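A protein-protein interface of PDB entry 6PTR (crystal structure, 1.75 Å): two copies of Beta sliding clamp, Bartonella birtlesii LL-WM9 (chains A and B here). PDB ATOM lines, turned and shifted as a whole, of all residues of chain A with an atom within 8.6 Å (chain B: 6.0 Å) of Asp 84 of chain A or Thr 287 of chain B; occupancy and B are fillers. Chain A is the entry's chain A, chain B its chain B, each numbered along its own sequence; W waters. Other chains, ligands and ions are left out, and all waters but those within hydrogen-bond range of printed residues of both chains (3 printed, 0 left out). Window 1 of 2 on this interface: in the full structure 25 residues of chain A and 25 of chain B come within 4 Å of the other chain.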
ATOM      1  N   ARG A  15     -19.932  34.668 -14.339  1.00  0.00           N
ATOM      2  CA  ARG A  15     -18.486  34.494 -14.191  1.00  0.00           C
ATOM      3  C   ARG A  15     -17.776  35.831 -14.078  1.00  0.00           C
ATOM      4  O   ARG A  15     -16.923  36.016 -13.200  1.00  0.00           O
ATOM      5  CB  ARG A  15     -17.921  33.681 -15.362  1.00  0.00           C
ATOM      6  CG  ARG A  15     -16.416  33.449 -15.297  1.00  0.00           C
ATOM      7  CD  ARG A  15     -15.648  34.545 -16.017  1.00  0.00           C
ATOM      8  NE  ARG A  15     -14.207  34.382 -15.895  1.00  0.00           N
ATOM      9  CZ  ARG A  15     -13.323  35.323 -16.204  1.00  0.00           C
ATOM     10  NH1 ARG A  15     -13.735  36.515 -16.638  1.00  0.00           N
ATOM     11  NH2 ARG A  15     -12.027  35.084 -16.068  1.00  0.00           N
ATOM     12  N   PHE A  19     -15.707  37.014 -10.911  1.00  0.00           N
ATOM     13  CA  PHE A  19     -14.261  37.187 -11.028  1.00  0.00           C
ATOM     14  C   PHE A  19     -13.844  38.567 -10.555  1.00  0.00           C
ATOM     15  O   PHE A  19     -12.861  38.705  -9.817  1.00  0.00           O
ATOM     16  CB  PHE A  19     -13.819  36.957 -12.476  1.00  0.00           C
ATOM     17  CG  PHE A  19     -12.325  36.929 -12.669  1.00  0.00           C
ATOM     18  CD1 PHE A  19     -11.532  36.035 -11.947  1.00  0.00           C
ATOM     19  CD2 PHE A  19     -11.717  37.749 -13.606  1.00  0.00           C
ATOM     20  CE1 PHE A  19     -10.161  35.995 -12.133  1.00  0.00           C
ATOM     21  CE2 PHE A  19     -10.349  37.712 -13.795  1.00  0.00           C
ATOM     22  CZ  PHE A  19      -9.570  36.834 -13.053  1.00  0.00           C
ATOM     23  N   LEU A  22     -14.304  38.674  -6.682  1.00  0.00           N
ATOM     24  CA  LEU A  22     -13.269  37.873  -6.034  1.00  0.00           C
ATOM     25  C   LEU A  22     -11.905  38.543  -6.165  1.00  0.00           C
ATOM     26  O   LEU A  22     -11.089  38.498  -5.236  1.00  0.00           O
ATOM     27  CB  LEU A  22     -13.251  36.468  -6.643  1.00  0.00           C
ATOM     28  CG  LEU A  22     -12.409  35.447  -5.899  1.00  0.00           C
ATOM     29  CD1 LEU A  22     -12.891  35.337  -4.459  1.00  0.00           C
ATOM     30  CD2 LEU A  22     -12.487  34.116  -6.616  1.00  0.00           C
ATOM     31  N   HIS A  26      -9.592  38.867  -2.779  1.00  0.00           N
ATOM     32  CA  HIS A  26      -8.621  37.807  -2.503  1.00  0.00           C
ATOM     33  C   HIS A  26      -7.230  38.368  -2.215  1.00  0.00           C
ATOM     34  O   HIS A  26      -6.424  37.688  -1.571  1.00  0.00           O
ATOM     35  CB  HIS A  26      -8.571  36.806  -3.668  1.00  0.00           C
ATOM     36  CG  HIS A  26      -7.653  37.209  -4.779  1.00  0.00           C
ATOM     37  ND1 HIS A  26      -7.927  38.262  -5.622  1.00  0.00           N
ATOM     38  CD2 HIS A  26      -6.466  36.700  -5.184  1.00  0.00           C
ATOM     39  CE1 HIS A  26      -6.941  38.396  -6.490  1.00  0.00           C
ATOM     40  NE2 HIS A  26      -6.048  37.450  -6.255  1.00  0.00           N
ATOM     41  N   PRO A  78     -10.370  28.129  -0.338  1.00  0.00           N
ATOM     42  CA  PRO A  78      -9.072  28.799  -0.535  1.00  0.00           C
ATOM     43  C   PRO A  78      -9.142  29.850  -1.632  1.00  0.00           C
ATOM     44  O   PRO A  78      -9.545  29.575  -2.761  1.00  0.00           O
ATOM     45  CB  PRO A  78      -8.139  27.648  -0.909  1.00  0.00           C
ATOM     46  CG  PRO A  78      -8.717  26.476  -0.161  1.00  0.00           C
ATOM     47  CD  PRO A  78     -10.209  26.662  -0.228  1.00  0.00           C
ATOM     48  N   ALA A  79      -8.717  31.074  -1.292  1.00  0.00           N
ATOM     49  CA  ALA A  79      -9.054  32.221  -2.127  1.00  0.00           C
ATOM     50  C   ALA A  79      -8.232  32.284  -3.405  1.00  0.00           C
ATOM     51  O   ALA A  79      -8.780  32.591  -4.476  1.00  0.00           O
ATOM     52  CB  ALA A  79      -8.884  33.508  -1.323  1.00  0.00           C
ATOM     53  N   TYR A  80      -6.918  32.052  -3.327  1.00  0.00           N
ATOM     54  CA  TYR A  80      -6.111  32.147  -4.538  1.00  0.00           C
ATOM     55  C   TYR A  80      -6.436  31.011  -5.498  1.00  0.00           C
ATOM     56  O   TYR A  80      -6.474  31.224  -6.713  1.00  0.00           O
ATOM     57  CB  TYR A  80      -4.621  32.150  -4.202  1.00  0.00           C
ATOM     58  CG  TYR A  80      -4.126  33.500  -3.721  1.00  0.00           C
ATOM     59  CD1 TYR A  80      -4.262  33.867  -2.393  1.00  0.00           C
ATOM     60  CD2 TYR A  80      -3.511  34.395  -4.589  1.00  0.00           C
ATOM     61  CE1 TYR A  80      -3.803  35.082  -1.930  1.00  0.00           C
ATOM     62  CE2 TYR A  80      -3.044  35.632  -4.127  1.00  0.00           C
ATOM     63  CZ  TYR A  80      -3.204  35.961  -2.791  1.00  0.00           C
ATOM     64  OH  TYR A  80      -2.767  37.167  -2.288  1.00  0.00           O
ATOM     65  N   LEU A  81      -6.682  29.803  -4.971  1.00  0.00           N
ATOM     66  CA  LEU A  81      -7.103  28.697  -5.827  1.00  0.00           C
ATOM     67  C   LEU A  81      -8.433  29.001  -6.502  1.00  0.00           C
ATOM     68  O   LEU A  81      -8.594  28.793  -7.707  1.00  0.00           O
ATOM     69  CB  LEU A  81      -7.210  27.402  -5.009  1.00  0.00           C
ATOM     70  CG  LEU A  81      -7.737  26.179  -5.783  1.00  0.00           C
ATOM     71  CD1 LEU A  81      -6.873  25.851  -7.009  1.00  0.00           C
ATOM     72  CD2 LEU A  81      -7.795  24.976  -4.824  1.00  0.00           C
ATOM     73  N   LEU A  82      -9.406  29.497  -5.744  1.00  0.00           N
ATOM     74  CA  LEU A  82     -10.679  29.825  -6.374  1.00  0.00           C
ATOM     75  C   LEU A  82     -10.498  30.885  -7.455  1.00  0.00           C
ATOM     76  O   LEU A  82     -11.081  30.777  -8.538  1.00  0.00           O
ATOM     77  CB  LEU A  82     -11.686  30.309  -5.333  1.00  0.00           C
ATOM     78  CG  LEU A  82     -13.073  30.631  -5.897  1.00  0.00           C
ATOM     79  CD1 LEU A  82     -13.757  29.420  -6.530  1.00  0.00           C
ATOM     80  CD2 LEU A  82     -13.941  31.221  -4.791  1.00  0.00           C
ATOM     81  N   TYR A  83      -9.725  31.934  -7.164  1.00  0.00           N
ATOM     82  CA  TYR A  83      -9.458  32.965  -8.155  1.00  0.00           C
ATOM     83  C   TYR A  83      -8.837  32.375  -9.410  1.00  0.00           C
ATOM     84  O   TYR A  83      -9.246  32.708 -10.527  1.00  0.00           O
ATOM     85  CB  TYR A  83      -8.519  34.013  -7.558  1.00  0.00           C
ATOM     86  CG  TYR A  83      -8.345  35.215  -8.413  1.00  0.00           C
ATOM     87  CD1 TYR A  83      -9.382  36.132  -8.563  1.00  0.00           C
ATOM     88  CD2 TYR A  83      -7.145  35.461  -9.059  1.00  0.00           C
ATOM     89  CE1 TYR A  83      -9.229  37.265  -9.334  1.00  0.00           C
ATOM     90  CE2 TYR A  83      -6.987  36.595  -9.847  1.00  0.00           C
ATOM     91  CZ  TYR A  83      -8.039  37.483  -9.975  1.00  0.00           C
ATOM     92  OH  TYR A  83      -7.907  38.615 -10.751  1.00  0.00           O
ATOM     93  N   ASP A  84      -7.839  31.496  -9.240  1.00  0.00           N
ATOM     94  CA  ASP A  84      -7.159  30.899 -10.388  1.00  0.00           C
ATOM     95  C   ASP A  84      -8.105  30.022 -11.203  1.00  0.00           C
ATOM     96  O   ASP A  84      -8.029  29.996 -12.435  1.00  0.00           O
ATOM     97  CB  ASP A  84      -5.945  30.088  -9.926  1.00  0.00           C
ATOM     98  CG  ASP A  84      -4.793  30.971  -9.441  1.00  0.00           C
ATOM     99  OD1 ASP A  84      -4.732  32.153  -9.830  1.00  0.00           O
ATOM    100  OD2 ASP A  84      -3.950  30.472  -8.672  1.00  0.00           O
ATOM    101  N   ILE A  85      -9.018  29.316 -10.530  1.00  0.00           N
ATOM    102  CA  ILE A  85     -10.033  28.535 -11.232  1.00  0.00           C
ATOM    103  C   ILE A  85     -10.943  29.454 -12.037  1.00  0.00           C
ATOM    104  O   ILE A  85     -11.168  29.242 -13.238  1.00  0.00           O
ATOM    105  CB  ILE A  85     -10.832  27.685 -10.231  1.00  0.00           C
ATOM    106  CG1 ILE A  85      -9.958  26.519  -9.746  1.00  0.00           C
ATOM    107  CG2 ILE A  85     -12.162  27.215 -10.863  1.00  0.00           C
ATOM    108  CD1 ILE A  85     -10.580  25.749  -8.541  1.00  0.00           C
ATOM    109  N   VAL A  86     -11.491  30.483 -11.389  1.00  0.00           N
ATOM    110  CA  VAL A  86     -12.448  31.344 -12.085  1.00  0.00           C
ATOM    111  C   VAL A  86     -11.786  32.088 -13.238  1.00  0.00           C
ATOM    112  O   VAL A  86     -12.414  32.325 -14.274  1.00  0.00           O
ATOM    113  CB  VAL A  86     -13.120  32.306 -11.086  1.00  0.00           C
ATOM    114  CG1 VAL A  86     -14.107  33.230 -11.829  1.00  0.00           C
ATOM    115  CG2 VAL A  86     -13.852  31.509 -10.028  1.00  0.00           C
ATOM    116  N   ARG A  87     -10.507  32.431 -13.095  1.00  0.00           N
ATOM    117  CA  ARG A  87      -9.776  33.074 -14.183  1.00  0.00           C
ATOM    118  C   ARG A  87      -9.885  32.276 -15.478  1.00  0.00           C
ATOM    119  O   ARG A  87     -10.020  32.849 -16.563  1.00  0.00           O
ATOM    120  CB  ARG A  87      -8.307  33.248 -13.783  1.00  0.00           C
ATOM    121  CG  ARG A  87      -7.461  33.946 -14.833  1.00  0.00           C
ATOM    122  CD  ARG A  87      -5.977  33.835 -14.531  1.00  0.00           C
ATOM    123  NE  ARG A  87      -5.503  34.868 -13.619  1.00  0.00           N
ATOM    124  CZ  ARG A  87      -4.890  34.628 -12.462  1.00  0.00           C
ATOM    125  NH1 ARG A  87      -4.673  33.379 -12.065  1.00  0.00           N
ATOM    126  NH2 ARG A  87      -4.486  35.639 -11.703  1.00  0.00           N
ATOM    127  N   LYS A  88      -9.841  30.944 -15.380  1.00  0.00           N
ATOM    128  CA  LYS A  88      -9.833  30.053 -16.535  1.00  0.00           C
ATOM    129  C   LYS A  88     -11.220  29.690 -17.040  1.00  0.00           C
ATOM    130  O   LYS A  88     -11.331  29.023 -18.078  1.00  0.00           O
ATOM    131  CB  LYS A  88      -9.104  28.753 -16.188  1.00  0.00           C
ATOM    132  CG  LYS A  88      -7.705  28.948 -15.675  1.00  0.00           C
ATOM    133  CD  LYS A  88      -6.963  27.599 -15.602  1.00  0.00           C
ATOM    134  CE  LYS A  88      -5.615  27.795 -14.941  1.00  0.00           C
ATOM    135  NZ  LYS A  88      -4.805  26.528 -14.881  1.00  0.00           N
ATOM    136  N   LEU A  89     -12.259  30.062 -16.323  1.00  0.00           N
ATOM    137  CA  LEU A  89     -13.606  29.770 -16.784  1.00  0.00           C
ATOM    138  C   LEU A  89     -14.037  30.826 -17.794  1.00  0.00           C
ATOM    139  O   LEU A  89     -13.684  31.998 -17.647  1.00  0.00           O
ATOM    140  CB  LEU A  89     -14.571  29.742 -15.612  1.00  0.00           C
ATOM    141  CG  LEU A  89     -14.255  28.625 -14.613  1.00  0.00           C
ATOM    142  CD1 LEU A  89     -15.285  28.626 -13.526  1.00  0.00           C
ATOM    143  CD2 LEU A  89     -14.213  27.286 -15.324  1.00  0.00           C
ATOM    144  N   THR A 114     -17.327  21.440 -16.766  1.00  0.00           N
ATOM    145  CA  THR A 114     -16.234  21.514 -15.807  1.00  0.00           C
ATOM    146  C   THR A 114     -16.803  21.475 -14.393  1.00  0.00           C
ATOM    147  O   THR A 114     -17.711  22.242 -14.067  1.00  0.00           O
ATOM    148  CB  THR A 114     -15.422  22.799 -16.015  1.00  0.00           C
ATOM    149  OG1 THR A 114     -15.167  23.010 -17.423  1.00  0.00           O
ATOM    150  CG2 THR A 114     -14.110  22.717 -15.280  1.00  0.00           C
ATOM    151  N   PHE A 116     -15.534  21.186 -10.277  1.00  0.00           N
ATOM    152  CA  PHE A 116     -14.554  21.085  -9.210  1.00  0.00           C
ATOM    153  C   PHE A 116     -15.250  20.715  -7.910  1.00  0.00           C
ATOM    154  O   PHE A 116     -16.370  21.157  -7.646  1.00  0.00           O
ATOM    155  CB  PHE A 116     -13.823  22.421  -8.983  1.00  0.00           C
ATOM    156  CG  PHE A 116     -13.034  22.896 -10.159  1.00  0.00           C
ATOM    157  CD1 PHE A 116     -13.639  23.643 -11.171  1.00  0.00           C
ATOM    158  CD2 PHE A 116     -11.677  22.589 -10.258  1.00  0.00           C
ATOM    159  CE1 PHE A 116     -12.893  24.080 -12.287  1.00  0.00           C
ATOM    160  CE2 PHE A 116     -10.926  23.028 -11.375  1.00  0.00           C
ATOM    161  CZ  PHE A 116     -11.541  23.767 -12.379  1.00  0.00           C
ATOM    162  N   LEU A 118     -13.960  21.279  -4.149  1.00  0.00           N
ATOM    163  CA  LEU A 118     -12.838  21.834  -3.398  1.00  0.00           C
ATOM    164  C   LEU A 118     -13.012  21.600  -1.905  1.00  0.00           C
ATOM    165  O   LEU A 118     -14.105  21.770  -1.366  1.00  0.00           O
ATOM    166  CB  LEU A 118     -12.689  23.339  -3.636  1.00  0.00           C
ATOM    167  CG  LEU A 118     -12.454  23.795  -5.086  1.00  0.00           C
ATOM    168  CD1 LEU A 118     -12.167  25.300  -5.078  1.00  0.00           C
ATOM    169  CD2 LEU A 118     -11.299  23.011  -5.654  1.00  0.00           C
ATOM    170  N   VAL B 282      -7.791  20.516 -20.023  1.00  0.00           N
ATOM    171  CA  VAL B 282      -6.665  20.075 -19.210  1.00  0.00           C
ATOM    172  C   VAL B 282      -6.170  21.221 -18.350  1.00  0.00           C
ATOM    173  O   VAL B 282      -5.871  21.041 -17.165  1.00  0.00           O
ATOM    174  CB  VAL B 282      -5.531  19.522 -20.099  1.00  0.00           C
ATOM    175  CG1 VAL B 282      -4.249  19.301 -19.270  1.00  0.00           C
ATOM    176  CG2 VAL B 282      -5.972  18.234 -20.777  1.00  0.00           C
ATOM    177  N   ASP B 283      -6.045  22.409 -18.945  1.00  0.00           N
ATOM    178  CA  ASP B 283      -5.647  23.589 -18.188  1.00  0.00           C
ATOM    179  C   ASP B 283      -6.586  23.810 -17.006  1.00  0.00           C
ATOM    180  O   ASP B 283      -6.137  24.024 -15.872  1.00  0.00           O
ATOM    181  CB  ASP B 283      -5.615  24.810 -19.125  1.00  0.00           C
ATOM    182  CG  ASP B 283      -5.012  26.041 -18.469  1.00  0.00           C
ATOM    183  OD1 ASP B 283      -4.230  25.883 -17.503  1.00  0.00           O
ATOM    184  OD2 ASP B 283      -5.314  27.170 -18.926  1.00  0.00           O
ATOM    185  N   ARG B 284      -7.898  23.717 -17.239  1.00  0.00           N
ATOM    186  CA  ARG B 284      -8.847  23.960 -16.161  1.00  0.00           C
ATOM    187  C   ARG B 284      -8.686  22.945 -15.031  1.00  0.00           C
ATOM    188  O   ARG B 284      -8.527  23.332 -13.869  1.00  0.00           O
ATOM    189  CB  ARG B 284     -10.280  23.946 -16.703  1.00  0.00           C
ATOM    190  CG  ARG B 284     -10.594  25.174 -17.559  1.00  0.00           C
ATOM    191  CD  ARG B 284     -12.071  25.244 -17.915  1.00  0.00           C
ATOM    192  NE  ARG B 284     -12.546  24.114 -18.714  1.00  0.00           N
ATOM    193  CZ  ARG B 284     -12.625  24.101 -20.040  1.00  0.00           C
ATOM    194  NH1 ARG B 284     -12.237  25.157 -20.748  1.00  0.00           N
ATOM    195  NH2 ARG B 284     -13.115  23.032 -20.667  1.00  0.00           N
ATOM    196  N   VAL B 285      -8.715  21.641 -15.343  1.00  0.00           N
ATOM    197  CA  VAL B 285      -8.758  20.661 -14.253  1.00  0.00           C
ATOM    198  C   VAL B 285      -7.417  20.581 -13.546  1.00  0.00           C
ATOM    199  O   VAL B 285      -7.379  20.232 -12.360  1.00  0.00           O
ATOM    200  CB  VAL B 285      -9.243  19.264 -14.735  1.00  0.00           C
ATOM    201  CG1 VAL B 285     -10.684  19.346 -15.282  1.00  0.00           C
ATOM    202  CG2 VAL B 285      -8.314  18.684 -15.807  1.00  0.00           C
ATOM    203  N   SER B 286      -6.314  20.956 -14.209  1.00  0.00           N
ATOM    204  CA  SER B 286      -5.006  20.889 -13.559  1.00  0.00           C
ATOM    205  C   SER B 286      -4.761  22.054 -12.608  1.00  0.00           C
ATOM    206  O   SER B 286      -3.710  22.089 -11.951  1.00  0.00           O
ATOM    207  CB  SER B 286      -3.894  20.839 -14.609  1.00  0.00           C
ATOM    208  OG  SER B 286      -3.832  22.024 -15.365  1.00  0.00           O
ATOM    209  N   THR B 287      -5.699  23.001 -12.528  1.00  0.00           N
ATOM    210  CA  THR B 287      -5.508  24.150 -11.647  1.00  0.00           C
ATOM    211  C   THR B 287      -5.317  23.704 -10.203  1.00  0.00           C
ATOM    212  O   THR B 287      -4.652  24.404  -9.424  1.00  0.00           O
ATOM    213  CB  THR B 287      -6.707  25.100 -11.737  1.00  0.00           C
ATOM    214  OG1 THR B 287      -7.023  25.385 -13.114  1.00  0.00           O
ATOM    215  CG2 THR B 287      -6.426  26.438 -11.031  1.00  0.00           C
ATOM    216  N   ILE B 288      -5.892  22.553  -9.825  1.00  0.00           N
ATOM    217  CA  ILE B 288      -5.808  22.121  -8.424  1.00  0.00           C
ATOM    218  C   ILE B 288      -4.530  21.364  -8.108  1.00  0.00           C
ATOM    219  O   ILE B 288      -4.344  20.946  -6.956  1.00  0.00           O
ATOM    220  CB  ILE B 288      -7.020  21.242  -8.026  1.00  0.00           C
ATOM    221  CG1 ILE B 288      -7.040  19.974  -8.862  1.00  0.00           C
ATOM    222  CG2 ILE B 288      -8.327  21.987  -8.249  1.00  0.00           C
ATOM    223  CD1 ILE B 288      -8.079  18.949  -8.343  1.00  0.00           C
ATOM    224  N   SER B 289      -3.648  21.153  -9.083  1.00  0.00           N
ATOM    225  CA  SER B 289      -2.466  20.346  -8.805  1.00  0.00           C
ATOM    226  C   SER B 289      -1.408  21.167  -8.080  1.00  0.00           C
ATOM    227  O   SER B 289      -1.454  22.401  -8.058  1.00  0.00           O
ATOM    228  CB  SER B 289      -1.885  19.770 -10.098  1.00  0.00           C
ATOM    229  OG  SER B 289      -2.777  18.821 -10.652  1.00  0.00           O
HETATM  230  O   HOH W   1     -10.451  27.574 -20.000  1.00  0.00           O
HETATM  231  O   HOH W   2      -3.605  27.173  -9.164  1.00  0.00           O
HETATM  232  O   HOH W   3      -2.896  24.581 -14.329  1.00  0.00           O
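No position is printed for both chains.
Of the printed residues of chain B, Asp 84 of chain A touches Thr 287. Thr 287 of chain B touches just these residues of chain A: Leu 81 (3.6 Å), Asp 84 (3.8 Å), Ile 85 (3.8 Å) and Lys 88 (3.1 Å). Ser 286 of chain B touches none of the printed residues of chain A. Printed residues of chain A within 4 Å of Ile 288 of chain B: Phe 116. Of the printed residues of chain B, Leu 81 of chain A touches Thr 287. Printed residues of chain A within 4 Å of Asp 283 of chain B: Lys 88.
Among the printed residues, merely in contact across the chains: Leu 81 of chain A with Thr 287 of chain B (3.6 Å), Asp 84 of chain A with Thr 287 of chain B (3.8 Å), Ile 85 of chain A with Thr 287 of chain B (3.8 Å), Lys 88 of chain A with Arg 284 of chain B (3.9 Å), Leu 89 of chain A with Arg 284 of chain B (3.9 Å), Phe 116 of chain A with Arg 284 of chain B (3.4 Å) and Phe 116 of chain A with Ile 288 of chain B (3.95 Å).
NZ of Lys 88 of chain A lies within hydrogen-bond range of OG1 of Thr 287 of chain B (3.1 Å). The side-chain amino group (NZ) of Lys 88 of chain A lies within salt-bridge range of the side-chain carboxylate (OD1) of Asp 283 of chain B (2.8 Å). NE of Arg 284 of chain B sits at hydrogen-bond distance from OG1 of Thr 114 of chain A, 3.1 Å away.
Of the 8 printed residues of chain B, 4 touch a printed residue of chain A. Hydrophobic or aromatic side chains of chain B within 4 Å of the printed part of chain A: Ile 288. Of the 19 printed residues of chain A, 7 touch a printed residue of chain B. Printed residues of chain A that touch a printed residue of chain B: Leu 81, Asp 84, Ile 85, Lys 88, Leu 89, Thr 114 and Phe 116.
Water W1 bridges O of Lys 88 of chain A (2.6 Å) and NH1 of Arg 284 of chain B (3.1 Å). Water W3 bridges the side-chain amino group of Lys 88 of chain A (2.8 Å) and the side-chain hydroxyl of Ser 286 of chain B (2.9 Å). Water W2 bridges O of Thr 287 of chain B and OD2 of Asp 84 of chain A.
The guanidinium group of Arg 15 of chain A sits at hydrogen-bond distance from the backbone carbonyl oxygen of Leu 89 of chain A, 3.0 Å away. The side-chain hydroxyl (OG) of Ser 286 of chain B is in hydrogen-bond range of the backbone carbonyl oxygen (O) of Asp 283 of chain B. The side-chain carboxylate (OD1) of Asp 84 of chain A lies within salt-bridge range of the guanidinium group (NH1) of Arg 87 of chain A (2.5 Å). The backbone carbonyl oxygen (O) of Arg 284 of chain B is in hydrogen-bond range of the side-chain hydroxyl (OG1) of Thr 287 of chain B, 2.7 Å away. The backbone carbonyl oxygen (O) of Asp 283 of chain B lies within hydrogen-bond range of the side-chain hydroxyl (OG1) of Thr 287 of chain B (3.2 Å).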
